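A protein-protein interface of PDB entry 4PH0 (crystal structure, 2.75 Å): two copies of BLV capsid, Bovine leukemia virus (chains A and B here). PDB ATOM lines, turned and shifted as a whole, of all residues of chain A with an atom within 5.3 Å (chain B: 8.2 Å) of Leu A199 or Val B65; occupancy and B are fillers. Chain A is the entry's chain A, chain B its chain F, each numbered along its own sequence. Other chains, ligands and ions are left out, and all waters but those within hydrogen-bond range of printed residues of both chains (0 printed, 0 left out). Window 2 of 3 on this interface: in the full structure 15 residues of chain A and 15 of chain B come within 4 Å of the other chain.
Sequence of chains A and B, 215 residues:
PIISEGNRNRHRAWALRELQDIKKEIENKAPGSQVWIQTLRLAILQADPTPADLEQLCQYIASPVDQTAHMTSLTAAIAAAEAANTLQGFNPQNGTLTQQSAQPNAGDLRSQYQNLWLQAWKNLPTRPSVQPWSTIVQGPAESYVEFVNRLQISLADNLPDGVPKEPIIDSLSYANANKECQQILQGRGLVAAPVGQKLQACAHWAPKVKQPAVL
No position is printed for both chains.
OG of Ser B63 sits at hydrogen-bond distance from OD2 of Asp B66, 2.7 Å away. The backbone carbonyl oxygen of Pro B64 lies within hydrogen-bond range of the side-chain hydroxyl of Thr B68, at 2.8 Å.
The backbone NH of Val B65 sits at hydrogen-bond distance from the side-chain amide oxygen of Gln A152 (2.9 Å). The side-chain amide oxygen of Gln A152 sits close to the side-chain hydroxyl of Thr B68 (3.4 Å). The side-chain amide oxygen (OE1) of Gln A152 lies close to the backbone carbonyl oxygen (O) of Pro B64 (3.1 Å).
Hydrophobic or aromatic side chains of chain B within 4 Å of the printed part of chain A: Pro B64 and Val B65. Among the printed residues, no Asp or Glu carboxylate lies within 4 Å of a Lys or Arg side-chain nitrogen of the other chain.
Among the printed residues, merely in contact across the chains: Val A145 with Val B65 (3.2 Å), Val A148 with Val B65 (3.5 Å), Asn A149 with Ser B63 (3.7 Å), Asn A149 with Pro B64 (3.6 Å), Asn A149 with Val B65 (3.3 Å), Gly A196 with Thr B72 (3.9 Å), Leu A199 with Val B65 (3.6 Å) and Leu A199 with Thr B68 (3.9 Å).
Leu A199 touches just these residues of chain B: Val B65 and Thr B68. Of the printed residues of chain B, Gln A152 touches Pro B64 (2.9 Å), Val B65 (2.9 Å) and Thr B68 (2.2 Å). Of the printed residues of chain A, Ser B63 touches Asn A149. Of the printed residues of chain A, Pro B64 touches Asn A149 (3.6 Å) and Gln A152 (2.9 Å). Printed residues of chain B within 4 Å of Val A148: Val B65 (3.5 Å). Gln B67 touches none of the printed residues of chain A. The nearest residue of chain B that does not touch Leu A199 is Ala B69 (4.2 Å). The nearest printed residue of chain A that does not touch Val B65 is Tyr A144 (5.7 Å).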
ATOM      1  N   TYR A 144      -3.630 -33.946  37.429  1.00  0.00           N
ATOM      2  CA  TYR A 144      -2.842 -33.287  36.385  1.00  0.00           C
ATOM      3  C   TYR A 144      -3.419 -31.915  36.076  1.00  0.00           C
ATOM      4  O   TYR A 144      -2.684 -30.943  35.968  1.00  0.00           O
ATOM      5  CB  TYR A 144      -2.781 -34.152  35.127  1.00  0.00           C
ATOM      6  CG  TYR A 144      -1.839 -33.669  34.038  1.00  0.00           C
ATOM      7  CD1 TYR A 144      -0.467 -33.799  34.181  1.00  0.00           C
ATOM      8  CD2 TYR A 144      -2.321 -33.156  32.841  1.00  0.00           C
ATOM      9  CE1 TYR A 144       0.406 -33.387  33.187  1.00  0.00           C
ATOM     10  CE2 TYR A 144      -1.453 -32.746  31.833  1.00  0.00           C
ATOM     11  CZ  TYR A 144      -0.091 -32.865  32.017  1.00  0.00           C
ATOM     12  OH  TYR A 144       0.788 -32.465  31.043  1.00  0.00           O
ATOM     13  N   VAL A 145      -4.739 -31.839  35.952  1.00  0.00           N
ATOM     14  CA  VAL A 145      -5.431 -30.579  35.664  1.00  0.00           C
ATOM     15  C   VAL A 145      -5.118 -29.540  36.747  1.00  0.00           C
ATOM     16  O   VAL A 145      -4.926 -28.356  36.463  1.00  0.00           O
ATOM     17  CB  VAL A 145      -6.957 -30.801  35.551  1.00  0.00           C
ATOM     18  CG1 VAL A 145      -7.684 -29.517  35.211  1.00  0.00           C
ATOM     19  CG2 VAL A 145      -7.255 -31.895  34.539  1.00  0.00           C
ATOM     20  N   VAL A 148      -1.502 -28.674  36.206  1.00  0.00           N
ATOM     21  CA  VAL A 148      -1.433 -27.765  35.076  1.00  0.00           C
ATOM     22  C   VAL A 148      -1.908 -26.383  35.488  1.00  0.00           C
ATOM     23  O   VAL A 148      -1.372 -25.377  35.029  1.00  0.00           O
ATOM     24  CB  VAL A 148      -2.250 -28.270  33.878  1.00  0.00           C
ATOM     25  CG1 VAL A 148      -2.243 -27.255  32.756  1.00  0.00           C
ATOM     26  CG2 VAL A 148      -1.680 -29.574  33.385  1.00  0.00           C
ATOM     27  N   ASN A 149      -2.896 -26.323  36.370  1.00  0.00           N
ATOM     28  CA  ASN A 149      -3.393 -25.027  36.816  1.00  0.00           C
ATOM     29  C   ASN A 149      -2.294 -24.193  37.479  1.00  0.00           C
ATOM     30  O   ASN A 149      -2.010 -23.083  37.037  1.00  0.00           O
ATOM     31  CB  ASN A 149      -4.580 -25.205  37.763  1.00  0.00           C
ATOM     32  CG  ASN A 149      -5.669 -24.179  37.523  1.00  0.00           C
ATOM     33  OD1 ASN A 149      -5.910 -23.774  36.384  1.00  0.00           O
ATOM     34  ND2 ASN A 149      -6.335 -23.756  38.593  1.00  0.00           N
ATOM     35  N   GLN A 152       0.286 -22.908  34.882  1.00  0.00           N
ATOM     36  CA  GLN A 152      -0.104 -21.808  34.011  1.00  0.00           C
ATOM     37  C   GLN A 152      -0.279 -20.463  34.702  1.00  0.00           C
ATOM     38  O   GLN A 152       0.066 -19.420  34.144  1.00  0.00           O
ATOM     39  CB  GLN A 152      -1.402 -22.190  33.319  1.00  0.00           C
ATOM     40  CG  GLN A 152      -1.189 -22.982  32.055  1.00  0.00           C
ATOM     41  CD  GLN A 152      -2.491 -23.396  31.420  1.00  0.00           C
ATOM     42  OE1 GLN A 152      -3.477 -23.644  32.112  1.00  0.00           O
ATOM     43  NE2 GLN A 152      -2.507 -23.467  30.097  1.00  0.00           N
ATOM     44  N   VAL A 195       0.805 -29.168  25.559  1.00  0.00           N
ATOM     45  CA  VAL A 195       0.207 -29.628  26.802  1.00  0.00           C
ATOM     46  C   VAL A 195      -1.272 -29.951  26.684  1.00  0.00           C
ATOM     47  O   VAL A 195      -1.765 -30.844  27.365  1.00  0.00           O
ATOM     48  CB  VAL A 195       0.393 -28.585  27.901  1.00  0.00           C
ATOM     49  CG1 VAL A 195      -0.248 -27.298  27.475  1.00  0.00           C
ATOM     50  CG2 VAL A 195      -0.200 -29.065  29.203  1.00  0.00           C
ATOM     51  N   GLY A 196      -1.976 -29.249  25.804  1.00  0.00           N
ATOM     52  CA  GLY A 196      -3.404 -29.460  25.678  1.00  0.00           C
ATOM     53  C   GLY A 196      -3.694 -30.896  25.317  1.00  0.00           C
ATOM     54  O   GLY A 196      -4.702 -31.456  25.739  1.00  0.00           O
ATOM     55  N   GLN A 197      -2.780 -31.506  24.570  1.00  0.00           N
ATOM     56  CA  GLN A 197      -2.933 -32.899  24.186  1.00  0.00           C
ATOM     57  C   GLN A 197      -2.390 -33.785  25.280  1.00  0.00           C
ATOM     58  O   GLN A 197      -2.761 -34.952  25.385  1.00  0.00           O
ATOM     59  CB  GLN A 197      -2.295 -33.162  22.834  1.00  0.00           C
ATOM     60  CG  GLN A 197      -3.012 -32.339  21.778  1.00  0.00           C
ATOM     61  CD  GLN A 197      -2.526 -32.581  20.381  1.00  0.00           C
ATOM     62  OE1 GLN A 197      -1.428 -33.096  20.171  1.00  0.00           O
ATOM     63  NE2 GLN A 197      -3.342 -32.199  19.403  1.00  0.00           N
ATOM     64  N   LYS A 198      -1.495 -33.226  26.083  1.00  0.00           N
ATOM     65  CA  LYS A 198      -1.049 -33.911  27.280  1.00  0.00           C
ATOM     66  C   LYS A 198      -2.239 -33.931  28.242  1.00  0.00           C
ATOM     67  O   LYS A 198      -2.476 -34.921  28.933  1.00  0.00           O
ATOM     68  CB  LYS A 198       0.147 -33.206  27.923  1.00  0.00           C
ATOM     69  CG  LYS A 198       1.451 -33.277  27.147  1.00  0.00           C
ATOM     70  CD  LYS A 198       2.571 -32.566  27.906  1.00  0.00           C
ATOM     71  CE  LYS A 198       3.926 -32.826  27.276  1.00  0.00           C
ATOM     72  NZ  LYS A 198       4.251 -31.898  26.167  1.00  0.00           N
ATOM     73  N   LEU A 199      -2.980 -32.823  28.280  1.00  0.00           N
ATOM     74  CA  LEU A 199      -4.170 -32.709  29.125  1.00  0.00           C
ATOM     75  C   LEU A 199      -5.224 -33.737  28.766  1.00  0.00           C
ATOM     76  O   LEU A 199      -5.750 -34.445  29.622  1.00  0.00           O
ATOM     77  CB  LEU A 199      -4.795 -31.321  28.991  1.00  0.00           C
ATOM     78  CG  LEU A 199      -4.259 -30.146  29.789  1.00  0.00           C
ATOM     79  CD1 LEU A 199      -4.860 -28.879  29.233  1.00  0.00           C
ATOM     80  CD2 LEU A 199      -4.580 -30.304  31.255  1.00  0.00           C
ATOM     81  N   GLN A 200      -5.508 -33.806  27.470  1.00  0.00           N
ATOM     82  CA  GLN A 200      -6.537 -34.673  26.922  1.00  0.00           C
ATOM     83  C   GLN A 200      -6.333 -36.092  27.409  1.00  0.00           C
ATOM     84  O   GLN A 200      -7.288 -36.816  27.673  1.00  0.00           O
ATOM     85  CB  GLN A 200      -6.517 -34.601  25.391  1.00  0.00           C
ATOM     86  CG  GLN A 200      -7.478 -35.534  24.672  1.00  0.00           C
ATOM     87  CD  GLN A 200      -7.758 -35.091  23.242  1.00  0.00           C
ATOM     88  OE1 GLN A 200      -7.344 -34.009  22.820  1.00  0.00           O
ATOM     89  NE2 GLN A 200      -8.440 -35.942  22.483  1.00  0.00           N
ATOM     90  N   ALA A 201      -5.073 -36.481  27.527  1.00  0.00           N
ATOM     91  CA  ALA A 201      -4.728 -37.823  27.940  1.00  0.00           C
ATOM     92  C   ALA A 201      -4.830 -38.068  29.449  1.00  0.00           C
ATOM     93  O   ALA A 201      -5.408 -39.062  29.875  1.00  0.00           O
ATOM     94  CB  ALA A 201      -3.339 -38.140  27.466  1.00  0.00           C
ATOM     95  N   CYS A 202      -4.282 -37.161  30.252  1.00  0.00           N
ATOM     96  CA  CYS A 202      -4.136 -37.391  31.697  1.00  0.00           C
ATOM     97  C   CYS A 202      -5.296 -36.971  32.593  1.00  0.00           C
ATOM     98  O   CYS A 202      -5.184 -37.037  33.822  1.00  0.00           O
ATOM     99  CB  CYS A 202      -2.900 -36.652  32.195  1.00  0.00           C
ATOM    100  SG  CYS A 202      -1.437 -36.983  31.267  1.00  0.00           S
ATOM    101  N   ALA A 203      -6.411 -36.571  31.998  1.00  0.00           N
ATOM    102  CA  ALA A 203      -7.514 -36.002  32.767  1.00  0.00           C
ATOM    103  C   ALA A 203      -8.244 -36.919  33.751  1.00  0.00           C
ATOM    104  O   ALA A 203      -8.916 -36.435  34.658  1.00  0.00           O
ATOM    105  CB  ALA A 203      -8.534 -35.419  31.787  1.00  0.00           C
ATOM    106  N   ALA B  62     -13.034 -18.833  32.754  1.00  0.00           N
ATOM    107  CA  ALA B  62     -12.419 -20.155  32.830  1.00  0.00           C
ATOM    108  C   ALA B  62     -11.049 -20.185  33.469  1.00  0.00           C
ATOM    109  O   ALA B  62     -10.249 -19.273  33.301  1.00  0.00           O
ATOM    110  CB  ALA B  62     -12.335 -20.755  31.447  1.00  0.00           C
ATOM    111  N   SER B  63     -10.776 -21.272  34.179  1.00  0.00           N
ATOM    112  CA  SER B  63      -9.449 -21.497  34.697  1.00  0.00           C
ATOM    113  C   SER B  63      -8.559 -21.704  33.495  1.00  0.00           C
ATOM    114  O   SER B  63      -9.005 -22.221  32.472  1.00  0.00           O
ATOM    115  CB  SER B  63      -9.397 -22.712  35.626  1.00  0.00           C
ATOM    116  OG  SER B  63      -9.716 -23.906  34.935  1.00  0.00           O
ATOM    117  N   PRO B  64      -7.299 -21.283  33.610  1.00  0.00           N
ATOM    118  CA  PRO B  64      -6.339 -21.344  32.511  1.00  0.00           C
ATOM    119  C   PRO B  64      -6.226 -22.730  31.883  1.00  0.00           C
ATOM    120  O   PRO B  64      -6.045 -22.820  30.673  1.00  0.00           O
ATOM    121  CB  PRO B  64      -5.030 -20.935  33.183  1.00  0.00           C
ATOM    122  CG  PRO B  64      -5.456 -20.057  34.303  1.00  0.00           C
ATOM    123  CD  PRO B  64      -6.722 -20.651  34.809  1.00  0.00           C
ATOM    124  N   VAL B  65      -6.362 -23.786  32.679  1.00  0.00           N
ATOM    125  CA  VAL B  65      -6.297 -25.142  32.144  1.00  0.00           C
ATOM    126  C   VAL B  65      -7.420 -25.317  31.157  1.00  0.00           C
ATOM    127  O   VAL B  65      -7.231 -25.788  30.039  1.00  0.00           O
ATOM    128  CB  VAL B  65      -6.448 -26.211  33.221  1.00  0.00           C
ATOM    129  CG1 VAL B  65      -6.524 -27.576  32.569  1.00  0.00           C
ATOM    130  CG2 VAL B  65      -5.288 -26.164  34.159  1.00  0.00           C
ATOM    131  N   ASP B  66      -8.601 -24.923  31.606  1.00  0.00           N
ATOM    132  CA  ASP B  66      -9.813 -25.047  30.833  1.00  0.00           C
ATOM    133  C   ASP B  66      -9.725 -24.160  29.592  1.00  0.00           C
ATOM    134  O   ASP B  66     -10.282 -24.471  28.545  1.00  0.00           O
ATOM    135  CB  ASP B  66     -11.005 -24.666  31.701  1.00  0.00           C
ATOM    136  CG  ASP B  66     -11.167 -25.592  32.898  1.00  0.00           C
ATOM    137  OD1 ASP B  66     -10.642 -26.725  32.860  1.00  0.00           O
ATOM    138  OD2 ASP B  66     -11.818 -25.184  33.882  1.00  0.00           O
ATOM    139  N   GLN B  67      -9.022 -23.042  29.730  1.00  0.00           N
ATOM    140  CA  GLN B  67      -8.755 -22.145  28.616  1.00  0.00           C
ATOM    141  C   GLN B  67      -7.941 -22.859  27.559  1.00  0.00           C
ATOM    142  O   GLN B  67      -8.170 -22.710  26.363  1.00  0.00           O
ATOM    143  CB  GLN B  67      -8.011 -20.915  29.093  1.00  0.00           C
ATOM    144  CG  GLN B  67      -8.770 -20.161  30.127  1.00  0.00           C
ATOM    145  CD  GLN B  67      -7.983 -19.004  30.644  1.00  0.00           C
ATOM    146  OE1 GLN B  67      -7.156 -18.433  29.931  1.00  0.00           O
ATOM    147  NE2 GLN B  67      -8.205 -18.663  31.906  1.00  0.00           N
ATOM    148  N   THR B  68      -6.955 -23.609  28.035  1.00  0.00           N
ATOM    149  CA  THR B  68      -6.018 -24.324  27.188  1.00  0.00           C
ATOM    150  C   THR B  68      -6.616 -25.455  26.375  1.00  0.00           C
ATOM    151  O   THR B  68      -6.420 -25.532  25.164  1.00  0.00           O
ATOM    152  CB  THR B  68      -4.922 -24.940  28.045  1.00  0.00           C
ATOM    153  OG1 THR B  68      -4.292 -23.915  28.816  1.00  0.00           O
ATOM    154  CG2 THR B  68      -3.904 -25.655  27.179  1.00  0.00           C
ATOM    155  N   ALA B  69      -7.341 -26.330  27.064  1.00  0.00           N
ATOM    156  CA  ALA B  69      -7.990 -27.499  26.470  1.00  0.00           C
ATOM    157  C   ALA B  69      -8.953 -27.157  25.339  1.00  0.00           C
ATOM    158  O   ALA B  69      -9.048 -27.874  24.342  1.00  0.00           O
ATOM    159  CB  ALA B  69      -8.723 -28.296  27.551  1.00  0.00           C
ATOM    160  N   HIS B  70      -9.664 -26.051  25.497  1.00  0.00           N
ATOM    161  CA  HIS B  70     -10.673 -25.653  24.532  1.00  0.00           C
ATOM    162  C   HIS B  70      -9.999 -25.350  23.182  1.00  0.00           C
ATOM    163  O   HIS B  70     -10.452 -25.821  22.137  1.00  0.00           O
ATOM    164  CB  HIS B  70     -11.473 -24.463  25.088  1.00  0.00           C
ATOM    165  CG  HIS B  70     -12.734 -24.156  24.335  1.00  0.00           C
ATOM    166  ND1 HIS B  70     -12.847 -23.101  23.457  1.00  0.00           N
ATOM    167  CD2 HIS B  70     -13.947 -24.760  24.349  1.00  0.00           C
ATOM    168  CE1 HIS B  70     -14.070 -23.070  22.957  1.00  0.00           C
ATOM    169  NE2 HIS B  70     -14.756 -24.068  23.479  1.00  0.00           N
ATOM    170  N   MET B  71      -8.893 -24.613  23.217  1.00  0.00           N
ATOM    171  CA  MET B  71      -8.171 -24.228  22.007  1.00  0.00           C
ATOM    172  C   MET B  71      -7.852 -25.411  21.099  1.00  0.00           C
ATOM    173  O   MET B  71      -7.900 -25.298  19.877  1.00  0.00           O
ATOM    174  CB  MET B  71      -6.859 -23.537  22.387  1.00  0.00           C
ATOM    175  CG  MET B  71      -6.979 -22.082  22.806  1.00  0.00           C
ATOM    176  SD  MET B  71      -7.543 -21.001  21.481  1.00  0.00           S
ATOM    177  CE  MET B  71      -6.265 -21.252  20.254  1.00  0.00           C
ATOM    178  N   THR B  72      -7.519 -26.540  21.712  1.00  0.00           N
ATOM    179  CA  THR B  72      -7.194 -27.768  20.984  1.00  0.00           C
ATOM    180  C   THR B  72      -8.366 -28.422  20.229  1.00  0.00           C
ATOM    181  O   THR B  72      -8.302 -28.605  19.009  1.00  0.00           O
ATOM    182  CB  THR B  72      -6.596 -28.817  21.942  1.00  0.00           C
ATOM    183  OG1 THR B  72      -5.346 -28.341  22.460  1.00  0.00           O
ATOM    184  CG2 THR B  72      -6.380 -30.139  21.217  1.00  0.00           C
ATOM    185  N   TRP B 121     -16.755 -27.308  24.360  1.00  0.00           N
ATOM    186  CA  TRP B 121     -16.869 -27.419  25.810  1.00  0.00           C
ATOM    187  C   TRP B 121     -17.372 -28.770  26.301  1.00  0.00           C
ATOM    188  O   TRP B 121     -17.310 -29.065  27.492  1.00  0.00           O
ATOM    189  CB  TRP B 121     -17.783 -26.333  26.339  1.00  0.00           C
ATOM    190  CG  TRP B 121     -17.210 -25.004  26.110  1.00  0.00           C
ATOM    191  CD1 TRP B 121     -17.544 -24.137  25.119  1.00  0.00           C
ATOM    192  CD2 TRP B 121     -16.144 -24.389  26.846  1.00  0.00           C
ATOM    193  NE1 TRP B 121     -16.780 -22.998  25.211  1.00  0.00           N
ATOM    194  CE2 TRP B 121     -15.907 -23.129  26.261  1.00  0.00           C
ATOM    195  CE3 TRP B 121     -15.378 -24.774  27.952  1.00  0.00           C
ATOM    196  CZ2 TRP B 121     -14.932 -22.255  26.739  1.00  0.00           C
ATOM    197  CZ3 TRP B 121     -14.412 -23.904  28.421  1.00  0.00           C
ATOM    198  CH2 TRP B 121     -14.198 -22.660  27.815  1.00  0.00           C
ATOM    199  N   LEU B 124     -14.709 -32.423  28.035  1.00  0.00           N
ATOM    200  CA  LEU B 124     -13.297 -32.092  28.184  1.00  0.00           C
ATOM    201  C   LEU B 124     -13.258 -31.704  29.640  1.00  0.00           C
ATOM    202  O   LEU B 124     -14.310 -31.773  30.266  1.00  0.00           O
ATOM    203  CB  LEU B 124     -12.840 -31.031  27.191  1.00  0.00           C
ATOM    204  CG  LEU B 124     -12.784 -31.627  25.787  1.00  0.00           C
ATOM    205  CD1 LEU B 124     -12.344 -30.580  24.808  1.00  0.00           C
ATOM    206  CD2 LEU B 124     -11.817 -32.815  25.764  1.00  0.00           C
ATOM    207  N   PRO B 125     -12.117 -31.249  30.199  1.00  0.00           N
ATOM    208  CA  PRO B 125     -11.836 -31.873  31.502  1.00  0.00           C
ATOM    209  C   PRO B 125     -12.827 -31.595  32.635  1.00  0.00           C
ATOM    210  O   PRO B 125     -12.445 -31.236  33.747  1.00  0.00           O
ATOM    211  CB  PRO B 125     -10.478 -31.258  31.885  1.00  0.00           C
ATOM    212  CG  PRO B 125      -9.947 -30.629  30.634  1.00  0.00           C
ATOM    213  CD  PRO B 125     -11.150 -30.184  29.890  1.00  0.00           C
